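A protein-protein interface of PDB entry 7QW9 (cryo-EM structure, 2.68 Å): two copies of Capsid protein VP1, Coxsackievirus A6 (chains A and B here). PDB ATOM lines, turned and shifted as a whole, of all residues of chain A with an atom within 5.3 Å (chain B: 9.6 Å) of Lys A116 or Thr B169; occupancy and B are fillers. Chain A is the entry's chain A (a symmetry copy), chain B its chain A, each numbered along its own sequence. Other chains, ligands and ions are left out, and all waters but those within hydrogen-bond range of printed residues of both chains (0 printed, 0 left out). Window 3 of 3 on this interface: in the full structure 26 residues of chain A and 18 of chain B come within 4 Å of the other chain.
The backbone NH of Gln A112 is in hydrogen-bond range of the side-chain amide oxygen of Gln B166. N of Ala B168 lies within hydrogen-bond range of OE1 of Gln A112, at 3.3 Å. The backbone carbonyl oxygen (O) of Arg A81 lies close to the backbone carbonyl oxygen (O) of Ala B168. The backbone carbonyl oxygen of Thr B169 lies close to the guanidinium group of Arg A81, 3.5 Å away. The backbone carbonyl oxygen (O) of Ala B168 is in hydrogen-bond range of the side-chain amino group (NZ) of Lys A116 (3.4 Å).
O of Lys A116 is in hydrogen-bond range of OH of Tyr A79, at 2.7 Å. O of Phe A78 sits at hydrogen-bond distance from NZ of Lys A116, 2.8 Å away.
Gln B166 touches Val A111. NE2 of Gln A112 touches CE2 of Tyr B163 (3.8 Å). OE1 of Gln A112 touches N of Thr B167, 3.7 Å away. N of Gln A113 touches CB of Ala B168, at 3.9 Å. Thr B169 touches Lys A116 (OG1 to CD, 3.3 Å).
Of chain B, only Ala B168 (3.4 Å) and Thr B169 (3.3 Å) come within 4 Å of Lys A116. Thr B169 touches just these residues of chain A: Arg A81 and Lys A116. Of chain B, only Ala B168 (3.3 Å) and Thr B169 (3.4 Å) come within 4 Å of Arg A81. Of the printed residues of chain A, Tyr B163 touches Gln A112. Printed residues of chain A within 4 Å of Gln B166: Val A111 (3.8 Å) and Gln A112 (3.4 Å). The nearest residue of chain A that does not touch Thr B169 is Gln A112 (4.7 Å). The nearest printed residue of chain B that does not touch Gln A113 is Gln B166 (5.0 Å).
Of the 14 printed residues of chain A, 5 touch a printed residue of chain B. Printed residues of chain A that touch a printed residue of chain B: Arg A81, Val A111, Gln A112, Gln A113 and Lys A116. Of the 16 printed residues of chain B, 5 touch a printed residue of chain A. Printed residues of chain B that touch a printed residue of chain A: Tyr B163, Gln B166, Thr B167, Ala B168 and Thr B169. Among the printed residues, no Asp or Glu carboxylate lies within 4 Å of a Lys or Arg side-chain nitrogen of the other chain.
No position is printed for both chains.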
ATOM      1  N   PHE A  78      31.862  26.249 -12.752  1.00  0.00           N
ATOM      2  CA  PHE A  78      30.473  26.711 -12.543  1.00  0.00           C
ATOM      3  C   PHE A  78      29.972  27.371 -13.818  1.00  0.00           C
ATOM      4  O   PHE A  78      28.841  27.078 -14.190  1.00  0.00           O
ATOM      5  CB  PHE A  78      30.395  27.693 -11.382  1.00  0.00           C
ATOM      6  CG  PHE A  78      28.999  28.125 -11.019  1.00  0.00           C
ATOM      7  CD1 PHE A  78      28.085  27.231 -10.519  1.00  0.00           C
ATOM      8  CD2 PHE A  78      28.614  29.438 -11.146  1.00  0.00           C
ATOM      9  CE1 PHE A  78      26.806  27.635 -10.191  1.00  0.00           C
ATOM     10  CE2 PHE A  78      27.343  29.847 -10.794  1.00  0.00           C
ATOM     11  CZ  PHE A  78      26.439  28.945 -10.313  1.00  0.00           C
ATOM     12  N   TYR A  79      30.786  28.197 -14.475  1.00  0.00           N
ATOM     13  CA  TYR A  79      30.355  29.069 -15.595  1.00  0.00           C
ATOM     14  C   TYR A  79      30.754  28.518 -16.958  1.00  0.00           C
ATOM     15  O   TYR A  79      30.102  28.942 -17.938  1.00  0.00           O
ATOM     16  CB  TYR A  79      30.991  30.442 -15.477  1.00  0.00           C
ATOM     17  CG  TYR A  79      30.360  31.317 -14.441  1.00  0.00           C
ATOM     18  CD1 TYR A  79      29.034  31.649 -14.531  1.00  0.00           C
ATOM     19  CD2 TYR A  79      31.090  31.833 -13.404  1.00  0.00           C
ATOM     20  CE1 TYR A  79      28.438  32.453 -13.591  1.00  0.00           C
ATOM     21  CE2 TYR A  79      30.511  32.636 -12.453  1.00  0.00           C
ATOM     22  CZ  TYR A  79      29.181  32.945 -12.549  1.00  0.00           C
ATOM     23  OH  TYR A  79      28.597  33.733 -11.611  1.00  0.00           O
ATOM     24  N   ARG A  81      30.097  26.458 -19.192  1.00  0.00           N
ATOM     25  CA  ARG A  81      28.986  25.598 -19.655  1.00  0.00           C
ATOM     26  C   ARG A  81      28.106  26.463 -20.556  1.00  0.00           C
ATOM     27  O   ARG A  81      27.556  27.458 -20.055  1.00  0.00           O
ATOM     28  CB  ARG A  81      28.152  25.099 -18.473  1.00  0.00           C
ATOM     29  CG  ARG A  81      28.868  24.165 -17.513  1.00  0.00           C
ATOM     30  CD  ARG A  81      28.019  23.629 -16.379  1.00  0.00           C
ATOM     31  NE  ARG A  81      28.892  22.783 -15.590  1.00  0.00           N
ATOM     32  CZ  ARG A  81      29.131  21.504 -15.825  1.00  0.00           C
ATOM     33  NH1 ARG A  81      28.486  20.874 -16.791  1.00  0.00           N
ATOM     34  NH2 ARG A  81      30.001  20.841 -15.079  1.00  0.00           N
ATOM     35  N   VAL A 111      16.654  33.411 -17.959  1.00  0.00           N
ATOM     36  CA  VAL A 111      16.819  33.294 -16.483  1.00  0.00           C
ATOM     37  C   VAL A 111      18.047  32.448 -16.152  1.00  0.00           C
ATOM     38  O   VAL A 111      18.786  32.835 -15.243  1.00  0.00           O
ATOM     39  CB  VAL A 111      15.571  32.736 -15.780  1.00  0.00           C
ATOM     40  CG1 VAL A 111      14.456  33.759 -15.770  1.00  0.00           C
ATOM     41  CG2 VAL A 111      15.091  31.417 -16.363  1.00  0.00           C
ATOM     42  N   GLN A 112      18.250  31.318 -16.817  1.00  0.00           N
ATOM     43  CA  GLN A 112      19.148  30.289 -16.267  1.00  0.00           C
ATOM     44  C   GLN A 112      20.563  30.833 -16.286  1.00  0.00           C
ATOM     45  O   GLN A 112      21.300  30.562 -15.319  1.00  0.00           O
ATOM     46  CB  GLN A 112      19.006  28.979 -17.017  1.00  0.00           C
ATOM     47  CG  GLN A 112      17.751  28.237 -16.624  1.00  0.00           C
ATOM     48  CD  GLN A 112      18.001  26.756 -16.581  1.00  0.00           C
ATOM     49  OE1 GLN A 112      18.915  26.243 -17.226  1.00  0.00           O
ATOM     50  NE2 GLN A 112      17.174  26.062 -15.815  1.00  0.00           N
ATOM     51  N   GLN A 113      20.904  31.599 -17.320  1.00  0.00           N
ATOM     52  CA  GLN A 113      22.267  32.148 -17.534  1.00  0.00           C
ATOM     53  C   GLN A 113      22.359  33.445 -16.744  1.00  0.00           C
ATOM     54  O   GLN A 113      23.374  33.648 -16.079  1.00  0.00           O
ATOM     55  CB  GLN A 113      22.539  32.331 -19.027  1.00  0.00           C
ATOM     56  CG  GLN A 113      23.934  32.828 -19.352  1.00  0.00           C
ATOM     57  CD  GLN A 113      24.976  31.758 -19.170  1.00  0.00           C
ATOM     58  OE1 GLN A 113      25.502  31.552 -18.076  1.00  0.00           O
ATOM     59  NE2 GLN A 113      25.312  31.087 -20.256  1.00  0.00           N
ATOM     60  N   ARG A 114      21.333  34.285 -16.825  1.00  0.00           N
ATOM     61  CA  ARG A 114      21.276  35.589 -16.135  1.00  0.00           C
ATOM     62  C   ARG A 114      21.565  35.391 -14.664  1.00  0.00           C
ATOM     63  O   ARG A 114      22.403  36.107 -14.137  1.00  0.00           O
ATOM     64  CB  ARG A 114      19.907  36.245 -16.230  1.00  0.00           C
ATOM     65  CG  ARG A 114      19.970  37.700 -15.804  1.00  0.00           C
ATOM     66  CD  ARG A 114      18.640  38.338 -16.055  1.00  0.00           C
ATOM     67  NE  ARG A 114      18.585  39.686 -15.546  1.00  0.00           N
ATOM     68  CZ  ARG A 114      17.561  40.500 -15.738  1.00  0.00           C
ATOM     69  NH1 ARG A 114      16.525  40.114 -16.466  1.00  0.00           N
ATOM     70  NH2 ARG A 114      17.570  41.713 -15.214  1.00  0.00           N
ATOM     71  N   ARG A 115      20.842  34.478 -14.040  1.00  0.00           N
ATOM     72  CA  ARG A 115      20.848  34.264 -12.578  1.00  0.00           C
ATOM     73  C   ARG A 115      22.224  33.771 -12.154  1.00  0.00           C
ATOM     74  O   ARG A 115      22.722  34.265 -11.115  1.00  0.00           O
ATOM     75  CB  ARG A 115      19.767  33.270 -12.189  1.00  0.00           C
ATOM     76  CG  ARG A 115      19.678  33.073 -10.691  1.00  0.00           C
ATOM     77  CD  ARG A 115      18.526  32.170 -10.367  1.00  0.00           C
ATOM     78  NE  ARG A 115      18.233  32.154  -8.956  1.00  0.00           N
ATOM     79  CZ  ARG A 115      18.724  31.309  -8.083  1.00  0.00           C
ATOM     80  NH1 ARG A 115      19.597  30.381  -8.424  1.00  0.00           N
ATOM     81  NH2 ARG A 115      18.352  31.397  -6.832  1.00  0.00           N
ATOM     82  N   LYS A 116      22.831  32.859 -12.917  1.00  0.00           N
ATOM     83  CA  LYS A 116      24.209  32.390 -12.655  1.00  0.00           C
ATOM     84  C   LYS A 116      25.165  33.570 -12.680  1.00  0.00           C
ATOM     85  O   LYS A 116      25.912  33.686 -11.704  1.00  0.00           O
ATOM     86  CB  LYS A 116      24.683  31.386 -13.691  1.00  0.00           C
ATOM     87  CG  LYS A 116      24.148  29.985 -13.467  1.00  0.00           C
ATOM     88  CD  LYS A 116      24.620  29.035 -14.513  1.00  0.00           C
ATOM     89  CE  LYS A 116      26.076  28.682 -14.334  1.00  0.00           C
ATOM     90  NZ  LYS A 116      26.627  28.131 -15.596  1.00  0.00           N
ATOM     91  N   LEU A 117      25.158  34.381 -13.752  1.00  0.00           N
ATOM     92  CA  LEU A 117      26.130  35.485 -13.973  1.00  0.00           C
ATOM     93  C   LEU A 117      25.947  36.546 -12.902  1.00  0.00           C
ATOM     94  O   LEU A 117      26.960  37.150 -12.556  1.00  0.00           O
ATOM     95  CB  LEU A 117      25.977  36.106 -15.360  1.00  0.00           C
ATOM     96  CG  LEU A 117      26.390  35.198 -16.500  1.00  0.00           C
ATOM     97  CD1 LEU A 117      26.073  35.817 -17.830  1.00  0.00           C
ATOM     98  CD2 LEU A 117      27.865  34.890 -16.429  1.00  0.00           C
ATOM     99  N   GLU A 118      24.735  36.739 -12.381  1.00  0.00           N
ATOM    100  CA  GLU A 118      24.430  37.814 -11.409  1.00  0.00           C
ATOM    101  C   GLU A 118      24.806  37.362 -10.011  1.00  0.00           C
ATOM    102  O   GLU A 118      24.532  38.102  -9.073  1.00  0.00           O
ATOM    103  CB  GLU A 118      22.971  38.237 -11.503  1.00  0.00           C
ATOM    104  CG  GLU A 118      22.752  39.172 -12.670  1.00  0.00           C
ATOM    105  CD  GLU A 118      21.328  39.666 -12.835  1.00  0.00           C
ATOM    106  OE1 GLU A 118      20.412  38.988 -12.321  1.00  0.00           O
ATOM    107  OE2 GLU A 118      21.132  40.730 -13.476  1.00  0.00           O
ATOM    108  N   LEU A 119      25.429  36.206  -9.859  1.00  0.00           N
ATOM    109  CA  LEU A 119      26.056  35.818  -8.578  1.00  0.00           C
ATOM    110  C   LEU A 119      27.196  36.789  -8.321  1.00  0.00           C
ATOM    111  O   LEU A 119      27.424  37.093  -7.164  1.00  0.00           O
ATOM    112  CB  LEU A 119      26.558  34.379  -8.654  1.00  0.00           C
ATOM    113  CG  LEU A 119      27.404  33.928  -7.479  1.00  0.00           C
ATOM    114  CD1 LEU A 119      26.616  34.011  -6.194  1.00  0.00           C
ATOM    115  CD2 LEU A 119      27.891  32.522  -7.688  1.00  0.00           C
ATOM    116  N   SER A 120      27.887  37.250  -9.365  1.00  0.00           N
ATOM    117  CA  SER A 120      28.983  38.244  -9.276  1.00  0.00           C
ATOM    118  C   SER A 120      28.474  39.629  -9.618  1.00  0.00           C
ATOM    119  O   SER A 120      27.481  39.712 -10.371  1.00  0.00           O
ATOM    120  CB  SER A 120      30.064  37.901 -10.205  1.00  0.00           C
ATOM    121  OG  SER A 120      30.553  36.615  -9.905  1.00  0.00           O
ATOM    122  N   PHE A 260      21.942  35.301  -4.765  1.00  0.00           N
ATOM    123  CA  PHE A 260      21.168  34.715  -5.885  1.00  0.00           C
ATOM    124  C   PHE A 260      19.782  35.348  -5.847  1.00  0.00           C
ATOM    125  O   PHE A 260      19.161  35.365  -4.782  1.00  0.00           O
ATOM    126  CB  PHE A 260      21.147  33.192  -5.769  1.00  0.00           C
ATOM    127  CG  PHE A 260      22.315  32.508  -6.418  1.00  0.00           C
ATOM    128  CD1 PHE A 260      22.559  32.700  -7.760  1.00  0.00           C
ATOM    129  CD2 PHE A 260      23.128  31.640  -5.716  1.00  0.00           C
ATOM    130  CE1 PHE A 260      23.615  32.057  -8.385  1.00  0.00           C
ATOM    131  CE2 PHE A 260      24.187  30.999  -6.334  1.00  0.00           C
ATOM    132  CZ  PHE A 260      24.429  31.206  -7.669  1.00  0.00           C
ATOM    133  N   MET B 148      19.463  16.322 -23.570  1.00  0.00           N
ATOM    134  CA  MET B 148      19.885  17.005 -22.337  1.00  0.00           C
ATOM    135  C   MET B 148      19.883  16.033 -21.169  1.00  0.00           C
ATOM    136  O   MET B 148      18.806  15.554 -20.826  1.00  0.00           O
ATOM    137  CB  MET B 148      18.923  18.138 -22.018  1.00  0.00           C
ATOM    138  CG  MET B 148      19.303  18.885 -20.768  1.00  0.00           C
ATOM    139  SD  MET B 148      18.273  20.328 -20.594  1.00  0.00           S
ATOM    140  CE  MET B 148      16.724  19.583 -20.094  1.00  0.00           C
ATOM    141  N   TYR B 149      21.038  15.834 -20.538  1.00  0.00           N
ATOM    142  CA  TYR B 149      21.181  15.019 -19.314  1.00  0.00           C
ATOM    143  C   TYR B 149      20.645  15.865 -18.174  1.00  0.00           C
ATOM    144  O   TYR B 149      21.123  16.973 -18.053  1.00  0.00           O
ATOM    145  CB  TYR B 149      22.631  14.592 -19.056  1.00  0.00           C
ATOM    146  CG  TYR B 149      22.831  13.960 -17.705  1.00  0.00           C
ATOM    147  CD1 TYR B 149      21.983  12.972 -17.275  1.00  0.00           C
ATOM    148  CD2 TYR B 149      23.805  14.393 -16.836  1.00  0.00           C
ATOM    149  CE1 TYR B 149      22.090  12.438 -16.012  1.00  0.00           C
ATOM    150  CE2 TYR B 149      23.950  13.846 -15.579  1.00  0.00           C
ATOM    151  CZ  TYR B 149      23.092  12.857 -15.173  1.00  0.00           C
ATOM    152  OH  TYR B 149      23.193  12.328 -13.922  1.00  0.00           O
ATOM    153  N   VAL B 150      19.677  15.360 -17.417  1.00  0.00           N
ATOM    154  CA  VAL B 150      18.983  16.053 -16.297  1.00  0.00           C
ATOM    155  C   VAL B 150      19.353  15.298 -15.034  1.00  0.00           C
ATOM    156  O   VAL B 150      18.762  14.259 -14.752  1.00  0.00           O
ATOM    157  CB  VAL B 150      17.474  16.025 -16.517  1.00  0.00           C
ATOM    158  CG1 VAL B 150      16.730  16.783 -15.443  1.00  0.00           C
ATOM    159  CG2 VAL B 150      17.115  16.563 -17.875  1.00  0.00           C
ATOM    160  N   PRO B 151      20.382  15.731 -14.273  1.00  0.00           N
ATOM    161  CA  PRO B 151      20.773  15.046 -13.052  1.00  0.00           C
ATOM    162  C   PRO B 151      19.645  15.025 -12.038  1.00  0.00           C
ATOM    163  O   PRO B 151      18.758  15.870 -12.120  1.00  0.00           O
ATOM    164  CB  PRO B 151      21.908  15.907 -12.522  1.00  0.00           C
ATOM    165  CG  PRO B 151      22.485  16.520 -13.751  1.00  0.00           C
ATOM    166  CD  PRO B 151      21.274  16.852 -14.580  1.00  0.00           C
ATOM    167  N   ALA B 154      17.481  18.233 -10.861  1.00  0.00           N
ATOM    168  CA  ALA B 154      17.380  19.225 -11.953  1.00  0.00           C
ATOM    169  C   ALA B 154      15.932  19.205 -12.419  1.00  0.00           C
ATOM    170  O   ALA B 154      15.367  18.118 -12.538  1.00  0.00           O
ATOM    171  CB  ALA B 154      18.335  18.889 -13.085  1.00  0.00           C
ATOM    172  N   PRO B 155      15.284  20.363 -12.698  1.00  0.00           N
ATOM    173  CA  PRO B 155      13.910  20.369 -13.204  1.00  0.00           C
ATOM    174  C   PRO B 155      13.793  19.658 -14.564  1.00  0.00           C
ATOM    175  O   PRO B 155      14.632  19.911 -15.426  1.00  0.00           O
ATOM    176  CB  PRO B 155      13.607  21.866 -13.342  1.00  0.00           C
ATOM    177  CG  PRO B 155      14.968  22.479 -13.588  1.00  0.00           C
ATOM    178  CD  PRO B 155      15.845  21.719 -12.621  1.00  0.00           C
ATOM    179  N   TYR B 163      11.577  26.519 -20.341  1.00  0.00           N
ATOM    180  CA  TYR B 163      12.799  27.259 -19.962  1.00  0.00           C
ATOM    181  C   TYR B 163      13.889  26.245 -19.641  1.00  0.00           C
ATOM    182  O   TYR B 163      15.071  26.609 -19.678  1.00  0.00           O
ATOM    183  CB  TYR B 163      12.500  28.212 -18.810  1.00  0.00           C
ATOM    184  CG  TYR B 163      12.437  27.541 -17.473  1.00  0.00           C
ATOM    185  CD1 TYR B 163      11.271  26.969 -17.017  1.00  0.00           C
ATOM    186  CD2 TYR B 163      13.553  27.481 -16.669  1.00  0.00           C
ATOM    187  CE1 TYR B 163      11.213  26.349 -15.783  1.00  0.00           C
ATOM    188  CE2 TYR B 163      13.520  26.856 -15.440  1.00  0.00           C
ATOM    189  CZ  TYR B 163      12.344  26.293 -14.992  1.00  0.00           C
ATOM    190  OH  TYR B 163      12.309  25.679 -13.773  1.00  0.00           O
ATOM    191  N   GLN B 164      13.506  25.005 -19.332  1.00  0.00           N
ATOM    192  CA  GLN B 164      14.449  23.956 -18.877  1.00  0.00           C
ATOM    193  C   GLN B 164      15.432  23.588 -19.984  1.00  0.00           C
ATOM    194  O   GLN B 164      16.483  23.058 -19.629  1.00  0.00           O
ATOM    195  CB  GLN B 164      13.708  22.725 -18.375  1.00  0.00           C
ATOM    196  CG  GLN B 164      12.981  22.974 -17.062  1.00  0.00           C
ATOM    197  CD  GLN B 164      11.502  23.174 -17.237  1.00  0.00           C
ATOM    198  OE1 GLN B 164      10.980  23.161 -18.342  1.00  0.00           O
ATOM    199  NE2 GLN B 164      10.802  23.304 -16.127  1.00  0.00           N
ATOM    200  N   TRP B 165      15.152  23.913 -21.245  1.00  0.00           N
ATOM    201  CA  TRP B 165      16.038  23.597 -22.399  1.00  0.00           C
ATOM    202  C   TRP B 165      17.068  24.691 -22.631  1.00  0.00           C
ATOM    203  O   TRP B 165      17.714  24.637 -23.668  1.00  0.00           O
ATOM    204  CB  TRP B 165      15.236  23.427 -23.685  1.00  0.00           C
ATOM    205  CG  TRP B 165      14.206  22.361 -23.642  1.00  0.00           C
ATOM    206  CD1 TRP B 165      12.868  22.531 -23.538  1.00  0.00           C
ATOM    207  CD2 TRP B 165      14.426  20.957 -23.745  1.00  0.00           C
ATOM    208  NE1 TRP B 165      12.237  21.321 -23.536  1.00  0.00           N
ATOM    209  CE2 TRP B 165      13.170  20.340 -23.679  1.00  0.00           C
ATOM    210  CE3 TRP B 165      15.555  20.159 -23.900  1.00  0.00           C
ATOM    211  CZ2 TRP B 165      13.015  18.967 -23.744  1.00  0.00           C
ATOM    212  CZ3 TRP B 165      15.402  18.798 -23.953  1.00  0.00           C
ATOM    213  CH2 TRP B 165      14.150  18.218 -23.873  1.00  0.00           C
ATOM    214  N   GLN B 166      17.188  25.678 -21.766  1.00  0.00           N
ATOM    215  CA  GLN B 166      18.238  26.714 -21.899  1.00  0.00           C
ATOM    216  C   GLN B 166      19.593  26.095 -21.576  1.00  0.00           C
ATOM    217  O   GLN B 166      20.553  26.511 -22.213  1.00  0.00           O
ATOM    218  CB  GLN B 166      17.922  27.908 -21.006  1.00  0.00           C
ATOM    219  CG  GLN B 166      16.721  28.681 -21.511  1.00  0.00           C
ATOM    220  CD  GLN B 166      16.183  29.692 -20.536  1.00  0.00           C
ATOM    221  OE1 GLN B 166      16.740  29.942 -19.473  1.00  0.00           O
ATOM    222  NE2 GLN B 166      15.071  30.291 -20.907  1.00  0.00           N
ATOM    223  N   THR B 167      19.654  25.144 -20.642  1.00  0.00           N
ATOM    224  CA  THR B 167      20.850  24.337 -20.291  1.00  0.00           C
ATOM    225  C   THR B 167      21.978  25.267 -19.851  1.00  0.00           C
ATOM    226  O   THR B 167      23.060  25.154 -20.428  1.00  0.00           O
ATOM    227  CB  THR B 167      21.362  23.466 -21.456  1.00  0.00           C
ATOM    228  OG1 THR B 167      21.990  24.215 -22.498  1.00  0.00           O
ATOM    229  CG2 THR B 167      20.288  22.668 -22.146  1.00  0.00           C
ATOM    230  N   ALA B 168      21.763  26.180 -18.905  1.00  0.00           N
ATOM    231  CA  ALA B 168      22.870  27.015 -18.403  1.00  0.00           C
ATOM    232  C   ALA B 168      23.889  26.074 -17.772  1.00  0.00           C
ATOM    233  O   ALA B 168      25.087  26.320 -17.984  1.00  0.00           O
ATOM    234  CB  ALA B 168      22.400  28.047 -17.425  1.00  0.00           C
ATOM    235  N   THR B 169      23.433  25.028 -17.065  1.00  0.00           N
ATOM    236  CA  THR B 169      24.320  24.095 -16.324  1.00  0.00           C
ATOM    237  C   THR B 169      24.131  22.632 -16.751  1.00  0.00           C
ATOM    238  O   THR B 169      25.149  21.924 -16.811  1.00  0.00           O
ATOM    239  CB  THR B 169      24.143  24.309 -14.821  1.00  0.00           C
ATOM    240  OG1 THR B 169      24.287  25.702 -14.528  1.00  0.00           O
ATOM    241  CG2 THR B 169      25.145  23.512 -14.017  1.00  0.00           C
ATOM    242  N   ASN B 170      22.906  22.160 -16.983  1.00  0.00           N
ATOM    243  CA  ASN B 170      22.635  20.796 -17.519  1.00  0.00           C
ATOM    244  C   ASN B 170      23.459  20.560 -18.780  1.00  0.00           C
ATOM    245  O   ASN B 170      23.372  21.360 -19.706  1.00  0.00           O
ATOM    246  CB  ASN B 170      21.164  20.603 -17.872  1.00  0.00           C
ATOM    247  CG  ASN B 170      20.365  20.144 -16.684  1.00  0.00           C
ATOM    248  OD1 ASN B 170      20.890  20.133 -15.577  1.00  0.00           O
ATOM    249  ND2 ASN B 170      19.125  19.725 -16.895  1.00  0.00           N
ATOM    250  N   PRO B 171      24.250  19.470 -18.895  1.00  0.00           N
ATOM    251  CA  PRO B 171      24.916  19.138 -20.149  1.00  0.00           C
ATOM    252  C   PRO B 171      23.915  18.680 -21.216  1.00  0.00           C
ATOM    253  O   PRO B 171      23.184  17.743 -20.984  1.00  0.00           O
ATOM    254  CB  PRO B 171      25.835  17.963 -19.803  1.00  0.00           C
ATOM    255  CG  PRO B 171      25.814  17.871 -18.307  1.00  0.00           C
ATOM    256  CD  PRO B 171      24.485  18.446 -17.878  1.00  0.00           C
ATOM    257  N   SER B 172      23.900  19.320 -22.372  1.00  0.00           N
ATOM    258  CA  SER B 172      23.053  18.886 -23.501  1.00  0.00           C
ATOM    259  C   SER B 172      23.902  18.665 -24.751  1.00  0.00           C
ATOM    260  O   SER B 172      25.019  19.172 -24.784  1.00  0.00           O
ATOM    261  CB  SER B 172      22.000  19.882 -23.740  1.00  0.00           C
ATOM    262  OG  SER B 172      22.615  21.076 -24.161  1.00  0.00           O
